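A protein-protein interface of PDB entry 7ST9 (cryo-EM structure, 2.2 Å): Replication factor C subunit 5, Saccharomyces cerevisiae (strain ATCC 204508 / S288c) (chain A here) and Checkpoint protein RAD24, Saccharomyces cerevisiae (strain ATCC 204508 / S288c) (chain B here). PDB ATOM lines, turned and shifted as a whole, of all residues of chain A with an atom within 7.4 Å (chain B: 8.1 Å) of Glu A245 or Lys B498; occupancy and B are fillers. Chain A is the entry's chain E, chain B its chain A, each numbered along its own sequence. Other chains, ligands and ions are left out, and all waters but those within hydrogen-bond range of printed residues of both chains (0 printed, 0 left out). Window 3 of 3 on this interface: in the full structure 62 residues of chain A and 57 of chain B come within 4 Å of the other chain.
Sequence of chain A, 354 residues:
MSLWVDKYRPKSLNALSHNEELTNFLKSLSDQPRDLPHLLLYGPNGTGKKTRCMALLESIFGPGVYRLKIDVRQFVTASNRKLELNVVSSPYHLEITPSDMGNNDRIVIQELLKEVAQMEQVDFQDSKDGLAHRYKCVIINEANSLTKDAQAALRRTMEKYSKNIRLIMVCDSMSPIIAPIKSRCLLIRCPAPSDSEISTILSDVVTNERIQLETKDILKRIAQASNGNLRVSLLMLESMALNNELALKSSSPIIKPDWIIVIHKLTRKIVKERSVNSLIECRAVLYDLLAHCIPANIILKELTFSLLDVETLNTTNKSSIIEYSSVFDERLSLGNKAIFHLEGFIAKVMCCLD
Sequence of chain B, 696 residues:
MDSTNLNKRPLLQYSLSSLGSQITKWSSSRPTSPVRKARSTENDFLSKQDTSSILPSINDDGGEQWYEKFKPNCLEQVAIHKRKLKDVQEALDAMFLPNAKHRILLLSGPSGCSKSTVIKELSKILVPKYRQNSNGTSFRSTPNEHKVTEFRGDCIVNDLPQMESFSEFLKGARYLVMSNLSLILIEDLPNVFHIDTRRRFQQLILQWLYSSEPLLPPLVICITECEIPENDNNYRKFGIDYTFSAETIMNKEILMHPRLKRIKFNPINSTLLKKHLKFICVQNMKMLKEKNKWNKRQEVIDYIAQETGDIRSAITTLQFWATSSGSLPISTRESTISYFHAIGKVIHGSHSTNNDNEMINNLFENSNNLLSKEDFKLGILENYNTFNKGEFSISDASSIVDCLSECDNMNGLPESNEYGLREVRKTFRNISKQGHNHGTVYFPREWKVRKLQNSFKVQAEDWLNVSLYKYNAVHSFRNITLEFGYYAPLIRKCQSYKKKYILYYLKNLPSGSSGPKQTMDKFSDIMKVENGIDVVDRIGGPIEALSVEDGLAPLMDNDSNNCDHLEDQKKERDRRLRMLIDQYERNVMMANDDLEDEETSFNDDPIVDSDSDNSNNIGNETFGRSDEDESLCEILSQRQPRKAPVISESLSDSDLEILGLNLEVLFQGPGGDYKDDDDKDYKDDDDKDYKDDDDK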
ATOM      1  N   ILE A 211       1.898  15.631   3.499  1.00  0.00           N
ATOM      2  CA  ILE A 211       3.153  14.976   3.151  1.00  0.00           C
ATOM      3  C   ILE A 211       4.061  15.997   2.483  1.00  0.00           C
ATOM      4  O   ILE A 211       3.665  16.655   1.512  1.00  0.00           O
ATOM      5  CB  ILE A 211       2.910  13.767   2.231  1.00  0.00           C
ATOM      6  CG1 ILE A 211       1.900  12.805   2.859  1.00  0.00           C
ATOM      7  CG2 ILE A 211       4.216  13.040   1.950  1.00  0.00           C
ATOM      8  CD1 ILE A 211       1.326  11.814   1.880  1.00  0.00           C
ATOM      9  N   GLN A 212       5.278  16.134   3.001  1.00  0.00           N
ATOM     10  CA  GLN A 212       6.230  17.100   2.469  1.00  0.00           C
ATOM     11  C   GLN A 212       6.794  16.586   1.150  1.00  0.00           C
ATOM     12  O   GLN A 212       7.378  15.498   1.100  1.00  0.00           O
ATOM     13  CB  GLN A 212       7.351  17.351   3.476  1.00  0.00           C
ATOM     14  CG  GLN A 212       6.903  18.090   4.725  1.00  0.00           C
ATOM     15  CD  GLN A 212       8.059  18.441   5.641  1.00  0.00           C
ATOM     16  OE1 GLN A 212       9.076  17.747   5.670  1.00  0.00           O
ATOM     17  NE2 GLN A 212       7.908  19.523   6.396  1.00  0.00           N
ATOM     18  N   SER A 239       2.765   3.922  -0.582  1.00  0.00           N
ATOM     19  CA  SER A 239       3.902   3.102  -0.172  1.00  0.00           C
ATOM     20  C   SER A 239       5.165   3.946  -0.037  1.00  0.00           C
ATOM     21  O   SER A 239       5.908   3.822   0.944  1.00  0.00           O
ATOM     22  CB  SER A 239       4.117   1.967  -1.174  1.00  0.00           C
ATOM     23  OG  SER A 239       3.033   1.055  -1.149  1.00  0.00           O
ATOM     24  N   MET A 240       5.423   4.816  -1.016  1.00  0.00           N
ATOM     25  CA  MET A 240       6.612   5.660  -0.968  1.00  0.00           C
ATOM     26  C   MET A 240       6.548   6.639   0.197  1.00  0.00           C
ATOM     27  O   MET A 240       7.557   6.876   0.870  1.00  0.00           O
ATOM     28  CB  MET A 240       6.770   6.410  -2.290  1.00  0.00           C
ATOM     29  CG  MET A 240       7.222   5.529  -3.445  1.00  0.00           C
ATOM     30  SD  MET A 240       7.019   6.315  -5.054  1.00  0.00           S
ATOM     31  CE  MET A 240       8.071   7.754  -4.866  1.00  0.00           C
ATOM     32  N   ALA A 241       5.373   7.223   0.450  1.00  0.00           N
ATOM     33  CA  ALA A 241       5.242   8.149   1.568  1.00  0.00           C
ATOM     34  C   ALA A 241       5.493   7.446   2.895  1.00  0.00           C
ATOM     35  O   ALA A 241       6.181   7.983   3.771  1.00  0.00           O
ATOM     36  CB  ALA A 241       3.857   8.793   1.555  1.00  0.00           C
ATOM     37  N   LEU A 242       4.944   6.240   3.066  1.00  0.00           N
ATOM     38  CA  LEU A 242       5.138   5.522   4.322  1.00  0.00           C
ATOM     39  C   LEU A 242       6.586   5.079   4.492  1.00  0.00           C
ATOM     40  O   LEU A 242       7.136   5.148   5.598  1.00  0.00           O
ATOM     41  CB  LEU A 242       4.196   4.322   4.393  1.00  0.00           C
ATOM     42  CG  LEU A 242       2.777   4.645   4.862  1.00  0.00           C
ATOM     43  CD1 LEU A 242       1.815   3.547   4.452  1.00  0.00           C
ATOM     44  CD2 LEU A 242       2.743   4.852   6.369  1.00  0.00           C
ATOM     45  N   ASN A 243       7.224   4.622   3.412  1.00  0.00           N
ATOM     46  CA  ASN A 243       8.600   4.147   3.502  1.00  0.00           C
ATOM     47  C   ASN A 243       9.612   5.276   3.642  1.00  0.00           C
ATOM     48  O   ASN A 243      10.776   5.000   3.951  1.00  0.00           O
ATOM     49  CB  ASN A 243       8.942   3.304   2.271  1.00  0.00           C
ATOM     50  CG  ASN A 243       8.546   1.850   2.429  1.00  0.00           C
ATOM     51  OD1 ASN A 243       9.127   1.121   3.233  1.00  0.00           O
ATOM     52  ND2 ASN A 243       7.550   1.421   1.664  1.00  0.00           N
ATOM     53  N   ASN A 244       9.205   6.527   3.425  1.00  0.00           N
ATOM     54  CA  ASN A 244      10.106   7.672   3.485  1.00  0.00           C
ATOM     55  C   ASN A 244       9.724   8.629   4.611  1.00  0.00           C
ATOM     56  O   ASN A 244      10.035   9.820   4.555  1.00  0.00           O
ATOM     57  CB  ASN A 244      10.127   8.406   2.145  1.00  0.00           C
ATOM     58  CG  ASN A 244      10.834   7.618   1.061  1.00  0.00           C
ATOM     59  OD1 ASN A 244      11.996   7.876   0.747  1.00  0.00           O
ATOM     60  ND2 ASN A 244      10.136   6.649   0.483  1.00  0.00           N
ATOM     61  N   GLU A 245       9.051   8.117   5.641  1.00  0.00           N
ATOM     62  CA  GLU A 245       8.659   8.924   6.796  1.00  0.00           C
ATOM     63  C   GLU A 245       7.802  10.115   6.372  1.00  0.00           C
ATOM     64  O   GLU A 245       7.907  11.210   6.930  1.00  0.00           O
ATOM     65  CB  GLU A 245       9.888   9.395   7.577  1.00  0.00           C
ATOM     66  CG  GLU A 245      10.892   8.294   7.879  1.00  0.00           C
ATOM     67  CD  GLU A 245      10.305   7.183   8.726  1.00  0.00           C
ATOM     68  OE1 GLU A 245       9.270   7.419   9.386  1.00  0.00           O
ATOM     69  OE2 GLU A 245      10.875   6.072   8.732  1.00  0.00           O
ATOM     70  N   LEU A 246       6.943   9.899   5.377  1.00  0.00           N
ATOM     71  CA  LEU A 246       6.036  10.934   4.883  1.00  0.00           C
ATOM     72  C   LEU A 246       6.794  12.177   4.425  1.00  0.00           C
ATOM     73  O   LEU A 246       6.315  13.303   4.582  1.00  0.00           O
ATOM     74  CB  LEU A 246       4.998  11.307   5.944  1.00  0.00           C
ATOM     75  CG  LEU A 246       4.209  10.141   6.541  1.00  0.00           C
ATOM     76  CD1 LEU A 246       3.339  10.616   7.693  1.00  0.00           C
ATOM     77  CD2 LEU A 246       3.364   9.458   5.475  1.00  0.00           C
ATOM     78  N   ALA A 247       7.983  11.984   3.853  1.00  0.00           N
ATOM     79  CA  ALA A 247       8.793  13.079   3.313  1.00  0.00           C
ATOM     80  C   ALA A 247       9.442  12.566   2.030  1.00  0.00           C
ATOM     81  O   ALA A 247      10.529  11.982   2.060  1.00  0.00           O
ATOM     82  CB  ALA A 247       9.829  13.557   4.322  1.00  0.00           C
ATOM     83  N   LEU A 248       8.770  12.789   0.905  1.00  0.00           N
ATOM     84  CA  LEU A 248       9.252  12.304  -0.378  1.00  0.00           C
ATOM     85  C   LEU A 248      10.385  13.181  -0.897  1.00  0.00           C
ATOM     86  O   LEU A 248      10.419  14.393  -0.668  1.00  0.00           O
ATOM     87  CB  LEU A 248       8.113  12.265  -1.396  1.00  0.00           C
ATOM     88  CG  LEU A 248       6.994  11.270  -1.080  1.00  0.00           C
ATOM     89  CD1 LEU A 248       5.704  11.672  -1.776  1.00  0.00           C
ATOM     90  CD2 LEU A 248       7.406   9.862  -1.477  1.00  0.00           C
ATOM     91  N   ILE B 491       1.883  -1.636   2.814  1.00  0.00           N
ATOM     92  CA  ILE B 491       1.383  -0.443   3.490  1.00  0.00           C
ATOM     93  C   ILE B 491       1.001  -0.771   4.927  1.00  0.00           C
ATOM     94  O   ILE B 491       1.327  -0.024   5.858  1.00  0.00           O
ATOM     95  CB  ILE B 491       0.197   0.148   2.708  1.00  0.00           C
ATOM     96  CG1 ILE B 491       0.695   0.849   1.442  1.00  0.00           C
ATOM     97  CG2 ILE B 491      -0.601   1.108   3.582  1.00  0.00           C
ATOM     98  CD1 ILE B 491      -0.377   1.053   0.392  1.00  0.00           C
ATOM     99  N   ARG B 492       0.302  -1.889   5.129  1.00  0.00           N
ATOM    100  CA  ARG B 492      -0.127  -2.247   6.477  1.00  0.00           C
ATOM    101  C   ARG B 492       1.065  -2.582   7.365  1.00  0.00           C
ATOM    102  O   ARG B 492       1.070  -2.245   8.553  1.00  0.00           O
ATOM    103  CB  ARG B 492      -1.109  -3.416   6.423  1.00  0.00           C
ATOM    104  CG  ARG B 492      -2.386  -3.122   5.644  1.00  0.00           C
ATOM    105  CD  ARG B 492      -3.154  -1.943   6.229  1.00  0.00           C
ATOM    106  NE  ARG B 492      -4.398  -1.687   5.512  1.00  0.00           N
ATOM    107  CZ  ARG B 492      -5.162  -0.620   5.697  1.00  0.00           C
ATOM    108  NH1 ARG B 492      -4.840   0.320   6.572  1.00  0.00           N
ATOM    109  NH2 ARG B 492      -6.276  -0.488   4.982  1.00  0.00           N
ATOM    110  N   LYS B 493       2.085  -3.242   6.813  1.00  0.00           N
ATOM    111  CA  LYS B 493       3.284  -3.533   7.592  1.00  0.00           C
ATOM    112  C   LYS B 493       3.992  -2.251   8.009  1.00  0.00           C
ATOM    113  O   LYS B 493       4.420  -2.113   9.163  1.00  0.00           O
ATOM    114  CB  LYS B 493       4.223  -4.429   6.785  1.00  0.00           C
ATOM    115  CG  LYS B 493       5.572  -4.669   7.441  1.00  0.00           C
ATOM    116  CD  LYS B 493       6.327  -5.794   6.754  1.00  0.00           C
ATOM    117  CE  LYS B 493       5.886  -7.156   7.266  1.00  0.00           C
ATOM    118  NZ  LYS B 493       6.538  -8.271   6.528  1.00  0.00           N
ATOM    119  N   CYS B 494       4.130  -1.300   7.083  1.00  0.00           N
ATOM    120  CA  CYS B 494       4.753  -0.027   7.433  1.00  0.00           C
ATOM    121  C   CYS B 494       3.947   0.699   8.503  1.00  0.00           C
ATOM    122  O   CYS B 494       4.514   1.257   9.453  1.00  0.00           O
ATOM    123  CB  CYS B 494       4.897   0.846   6.185  1.00  0.00           C
ATOM    124  SG  CYS B 494       6.132   0.251   5.007  1.00  0.00           S
ATOM    125  N   GLN B 495       2.619   0.700   8.368  1.00  0.00           N
ATOM    126  CA  GLN B 495       1.776   1.360   9.359  1.00  0.00           C
ATOM    127  C   GLN B 495       1.908   0.696  10.723  1.00  0.00           C
ATOM    128  O   GLN B 495       1.953   1.379  11.751  1.00  0.00           O
ATOM    129  CB  GLN B 495       0.320   1.350   8.894  1.00  0.00           C
ATOM    130  CG  GLN B 495       0.037   2.307   7.747  1.00  0.00           C
ATOM    131  CD  GLN B 495      -1.408   2.267   7.297  1.00  0.00           C
ATOM    132  OE1 GLN B 495      -2.087   1.250   7.440  1.00  0.00           O
ATOM    133  NE2 GLN B 495      -1.887   3.376   6.745  1.00  0.00           N
ATOM    134  N   SER B 496       1.962  -0.638  10.754  1.00  0.00           N
ATOM    135  CA  SER B 496       2.119  -1.344  12.022  1.00  0.00           C
ATOM    136  C   SER B 496       3.465  -1.033  12.663  1.00  0.00           C
ATOM    137  O   SER B 496       3.552  -0.848  13.882  1.00  0.00           O
ATOM    138  CB  SER B 496       1.965  -2.849  11.803  1.00  0.00           C
ATOM    139  OG  SER B 496       2.087  -3.556  13.024  1.00  0.00           O
ATOM    140  N   TYR B 497       4.528  -0.982  11.858  1.00  0.00           N
ATOM    141  CA  TYR B 497       5.837  -0.631  12.401  1.00  0.00           C
ATOM    142  C   TYR B 497       5.824   0.775  12.988  1.00  0.00           C
ATOM    143  O   TYR B 497       6.350   1.008  14.084  1.00  0.00           O
ATOM    144  CB  TYR B 497       6.903  -0.749  11.313  1.00  0.00           C
ATOM    145  CG  TYR B 497       8.319  -0.640  11.831  1.00  0.00           C
ATOM    146  CD1 TYR B 497       8.913  -1.695  12.510  1.00  0.00           C
ATOM    147  CD2 TYR B 497       9.061   0.518  11.642  1.00  0.00           C
ATOM    148  CE1 TYR B 497      10.207  -1.600  12.986  1.00  0.00           C
ATOM    149  CE2 TYR B 497      10.356   0.622  12.114  1.00  0.00           C
ATOM    150  CZ  TYR B 497      10.924  -0.440  12.786  1.00  0.00           C
ATOM    151  OH  TYR B 497      12.212  -0.341  13.258  1.00  0.00           O
ATOM    152  N   LYS B 498       5.221   1.728  12.271  1.00  0.00           N
ATOM    153  CA  LYS B 498       5.135   3.090  12.788  1.00  0.00           C
ATOM    154  C   LYS B 498       4.316   3.141  14.070  1.00  0.00           C
ATOM    155  O   LYS B 498       4.666   3.861  15.012  1.00  0.00           O
ATOM    156  CB  LYS B 498       4.535   4.017  11.731  1.00  0.00           C
ATOM    157  CG  LYS B 498       4.633   5.493  12.085  1.00  0.00           C
ATOM    158  CD  LYS B 498       4.924   6.346  10.862  1.00  0.00           C
ATOM    159  CE  LYS B 498       5.181   7.795  11.244  1.00  0.00           C
ATOM    160  NZ  LYS B 498       5.859   8.551  10.155  1.00  0.00           N
ATOM    161  N   LYS B 499       3.212   2.390  14.122  1.00  0.00           N
ATOM    162  CA  LYS B 499       2.391   2.355  15.326  1.00  0.00           C
ATOM    163  C   LYS B 499       3.178   1.806  16.507  1.00  0.00           C
ATOM    164  O   LYS B 499       3.104   2.346  17.618  1.00  0.00           O
ATOM    165  CB  LYS B 499       1.139   1.511  15.076  1.00  0.00           C
ATOM    166  CG  LYS B 499       0.223   1.357  16.285  1.00  0.00           C
ATOM    167  CD  LYS B 499      -0.856   0.316  16.028  1.00  0.00           C
ATOM    168  CE  LYS B 499      -1.856   0.252  17.171  1.00  0.00           C
ATOM    169  NZ  LYS B 499      -2.756  -0.929  17.062  1.00  0.00           N
ATOM    170  N   LYS B 500       3.931   0.725  16.291  1.00  0.00           N
ATOM    171  CA  LYS B 500       4.732   0.159  17.370  1.00  0.00           C
ATOM    172  C   LYS B 500       5.788   1.149  17.844  1.00  0.00           C
ATOM    173  O   LYS B 500       6.008   1.305  19.052  1.00  0.00           O
ATOM    174  CB  LYS B 500       5.384  -1.145  16.911  1.00  0.00           C
ATOM    175  CG  LYS B 500       6.123  -1.885  18.014  1.00  0.00           C
ATOM    176  CD  LYS B 500       6.486  -3.299  17.589  1.00  0.00           C
ATOM    177  CE  LYS B 500       7.225  -4.037  18.692  1.00  0.00           C
ATOM    178  NZ  LYS B 500       7.470  -5.464  18.346  1.00  0.00           N
ATOM    179  N   TYR B 501       6.453   1.829  16.907  1.00  0.00           N
ATOM    180  CA  TYR B 501       7.461   2.811  17.294  1.00  0.00           C
ATOM    181  C   TYR B 501       6.841   3.952  18.092  1.00  0.00           C
ATOM    182  O   TYR B 501       7.404   4.394  19.101  1.00  0.00           O
ATOM    183  CB  TYR B 501       8.171   3.351  16.052  1.00  0.00           C
ATOM    184  CG  TYR B 501       9.031   4.565  16.323  1.00  0.00           C
ATOM    185  CD1 TYR B 501      10.181   4.467  17.094  1.00  0.00           C
ATOM    186  CD2 TYR B 501       8.692   5.808  15.807  1.00  0.00           C
ATOM    187  CE1 TYR B 501      10.970   5.573  17.344  1.00  0.00           C
ATOM    188  CE2 TYR B 501       9.475   6.920  16.051  1.00  0.00           C
ATOM    189  CZ  TYR B 501      10.613   6.797  16.821  1.00  0.00           C
ATOM    190  OH  TYR B 501      11.396   7.901  17.067  1.00  0.00           O
ATOM    191  N   ILE B 502       5.678   4.441  17.656  1.00  0.00           N
ATOM    192  CA  ILE B 502       5.021   5.538  18.361  1.00  0.00           C
ATOM    193  C   ILE B 502       4.590   5.096  19.754  1.00  0.00           C
ATOM    194  O   ILE B 502       4.721   5.850  20.724  1.00  0.00           O
ATOM    195  CB  ILE B 502       3.828   6.060  17.538  1.00  0.00           C
ATOM    196  CG1 ILE B 502       4.328   6.780  16.283  1.00  0.00           C
ATOM    197  CG2 ILE B 502       2.970   6.994  18.380  1.00  0.00           C
ATOM    198  CD1 ILE B 502       3.270   6.952  15.213  1.00  0.00           C
ATOM    199  N   LEU B 503       4.057   3.878  19.874  1.00  0.00           N
ATOM    200  CA  LEU B 503       3.659   3.377  21.185  1.00  0.00           C
ATOM    201  C   LEU B 503       4.862   3.247  22.109  1.00  0.00           C
ATOM    202  O   LEU B 503       4.786   3.596  23.293  1.00  0.00           O
ATOM    203  CB  LEU B 503       2.947   2.032  21.038  1.00  0.00           C
ATOM    204  CG  LEU B 503       1.486   2.089  20.585  1.00  0.00           C
ATOM    205  CD1 LEU B 503       0.973   0.694  20.266  1.00  0.00           C
ATOM    206  CD2 LEU B 503       0.613   2.751  21.641  1.00  0.00           C
ATOM    207  N   TYR B 504       5.984   2.743  21.587  1.00  0.00           N
ATOM    208  CA  TYR B 504       7.190   2.639  22.402  1.00  0.00           C
ATOM    209  C   TYR B 504       7.667   4.014  22.849  1.00  0.00           C
ATOM    210  O   TYR B 504       8.051   4.201  24.010  1.00  0.00           O
ATOM    211  CB  TYR B 504       8.287   1.915  21.619  1.00  0.00           C
ATOM    212  CG  TYR B 504       9.678   2.105  22.184  1.00  0.00           C
ATOM    213  CD1 TYR B 504      10.158   1.276  23.189  1.00  0.00           C
ATOM    214  CD2 TYR B 504      10.512   3.108  21.709  1.00  0.00           C
ATOM    215  CE1 TYR B 504      11.429   1.443  23.707  1.00  0.00           C
ATOM    216  CE2 TYR B 504      11.783   3.283  22.221  1.00  0.00           C
ATOM    217  CZ  TYR B 504      12.237   2.448  23.219  1.00  0.00           C
ATOM    218  OH  TYR B 504      13.502   2.619  23.731  1.00  0.00           O
ATOM    219  N   TYR B 505       7.649   4.993  21.940  1.00  0.00           N
ATOM    220  CA  TYR B 505       8.065   6.343  22.302  1.00  0.00           C
ATOM    221  C   TYR B 505       7.157   6.928  23.375  1.00  0.00           C
ATOM    222  O   TYR B 505       7.633   7.555  24.330  1.00  0.00           O
ATOM    223  CB  TYR B 505       8.075   7.236  21.061  1.00  0.00           C
ATOM    224  CG  TYR B 505       8.280   8.704  21.360  1.00  0.00           C
ATOM    225  CD1 TYR B 505       9.556   9.233  21.504  1.00  0.00           C
ATOM    226  CD2 TYR B 505       7.197   9.564  21.494  1.00  0.00           C
ATOM    227  CE1 TYR B 505       9.748  10.573  21.776  1.00  0.00           C
ATOM    228  CE2 TYR B 505       7.380  10.907  21.766  1.00  0.00           C
ATOM    229  CZ  TYR B 505       8.657  11.405  21.906  1.00  0.00           C
ATOM    230  OH  TYR B 505       8.843  12.742  22.177  1.00  0.00           O
ATOM    231  N   PHE B 523      -0.857  11.610  12.873  1.00  0.00           N
ATOM    232  CA  PHE B 523      -0.841  10.318  12.192  1.00  0.00           C
ATOM    233  C   PHE B 523      -2.019   9.452  12.611  1.00  0.00           C
ATOM    234  O   PHE B 523      -1.912   8.223  12.657  1.00  0.00           O
ATOM    235  CB  PHE B 523       0.471   9.590  12.468  1.00  0.00           C
ATOM    236  CG  PHE B 523       1.657  10.501  12.596  1.00  0.00           C
ATOM    237  CD1 PHE B 523       2.189  11.121  11.479  1.00  0.00           C
ATOM    238  CD2 PHE B 523       2.259  10.715  13.825  1.00  0.00           C
ATOM    239  CE1 PHE B 523       3.280  11.953  11.586  1.00  0.00           C
ATOM    240  CE2 PHE B 523       3.359  11.547  13.939  1.00  0.00           C
ATOM    241  CZ  PHE B 523       3.869  12.166  12.816  1.00  0.00           C
ATOM    242  N   ILE B 526      -2.726   5.956  11.400  1.00  0.00           N
ATOM    243  CA  ILE B 526      -1.698   4.920  11.395  1.00  0.00           C
ATOM    244  C   ILE B 526      -1.918   3.897  12.505  1.00  0.00           C
ATOM    245  O   ILE B 526      -1.727   2.700  12.284  1.00  0.00           O
ATOM    246  CB  ILE B 526      -0.295   5.556  11.480  1.00  0.00           C
ATOM    247  CG1 ILE B 526       0.178   5.941  10.076  1.00  0.00           C
ATOM    248  CG2 ILE B 526       0.701   4.599  12.128  1.00  0.00           C
ATOM    249  CD1 ILE B 526       1.302   6.951  10.047  1.00  0.00           C
ATOM    250  N   MET B 527      -2.322   4.319  13.708  1.00  0.00           N
ATOM    251  CA  MET B 527      -2.537   3.359  14.786  1.00  0.00           C
ATOM    252  C   MET B 527      -3.938   2.754  14.766  1.00  0.00           C
ATOM    253  O   MET B 527      -4.396   2.248  15.799  1.00  0.00           O
ATOM    254  CB  MET B 527      -2.275   3.972  16.171  1.00  0.00           C
ATOM    255  CG  MET B 527      -3.251   5.044  16.650  1.00  0.00           C
ATOM    256  SD  MET B 527      -3.612   6.390  15.503  1.00  0.00           S
ATOM    257  CE  MET B 527      -1.959   7.058  15.266  1.00  0.00           C
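The guanidinium group of Arg B492 sits at hydrogen-bond distance from the side-chain amide oxygen of Gln B495 (3.0 Å).
O of Ala A241 lies within hydrogen-bond range of N of Leu A246 (2.6 Å).
N of Gln A212 is in hydrogen-bond range of O of Leu A246.
O of Ser A239 is in hydrogen-bond range of ND2 of Asn A243.
Of the 18 printed residues of chain B, 5 touch a printed residue of chain A.
Hydrophobic or aromatic side chains of chain B within 4 Å of the printed part of chain A: Ile B491 and Phe B523.
Among the printed residues, 7 pairs touch across the chains.
Among the printed residues, Asp or Glu carboxylates within 4 Å of a Lys or Arg side-chain nitrogen of the other chain: Glu A245 with Lys B498 (3.7 Å).
Of the printed residues of chain B, Leu A242 touches Ile B491 (3.5 Å), Cys B494 (3.97 Å) and Gln B495 (3.9 Å).
Lys B493 touches none of the printed residues of chain A.
Of the printed residues of chain A, Cys B494 touches Leu A242 (3.97 Å) and Asn A243 (3.6 Å).
Of the printed residues of chain A, Phe B523 touches Leu A246 (3.99 Å).
The nearest residue of chain B that does not touch Glu A245 is Tyr B497 (6.4 Å).
The nearest printed residue of chain A that does not touch Cys B494 is Ser A239 (5.4 Å).
NZ of Lys B498 is in salt-bridge range of OE1 of Glu A245, 3.7 Å away.
The side-chain sulfur (SG) of Cys B494 is in hydrogen-bond range of the side-chain amide oxygen (OD1) of Asn A243 (3.6 Å).
Among the printed residues, pairs that only touch across the chains: Ser A239 with Ile B491 (3.5 Å), Leu A242 with Ile B491 (3.5 Å), Leu A242 with Gln B495 (3.9 Å), Leu A242 with Cys B494 (3.97 Å) and Leu A246 with Phe B523 (3.99 Å).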
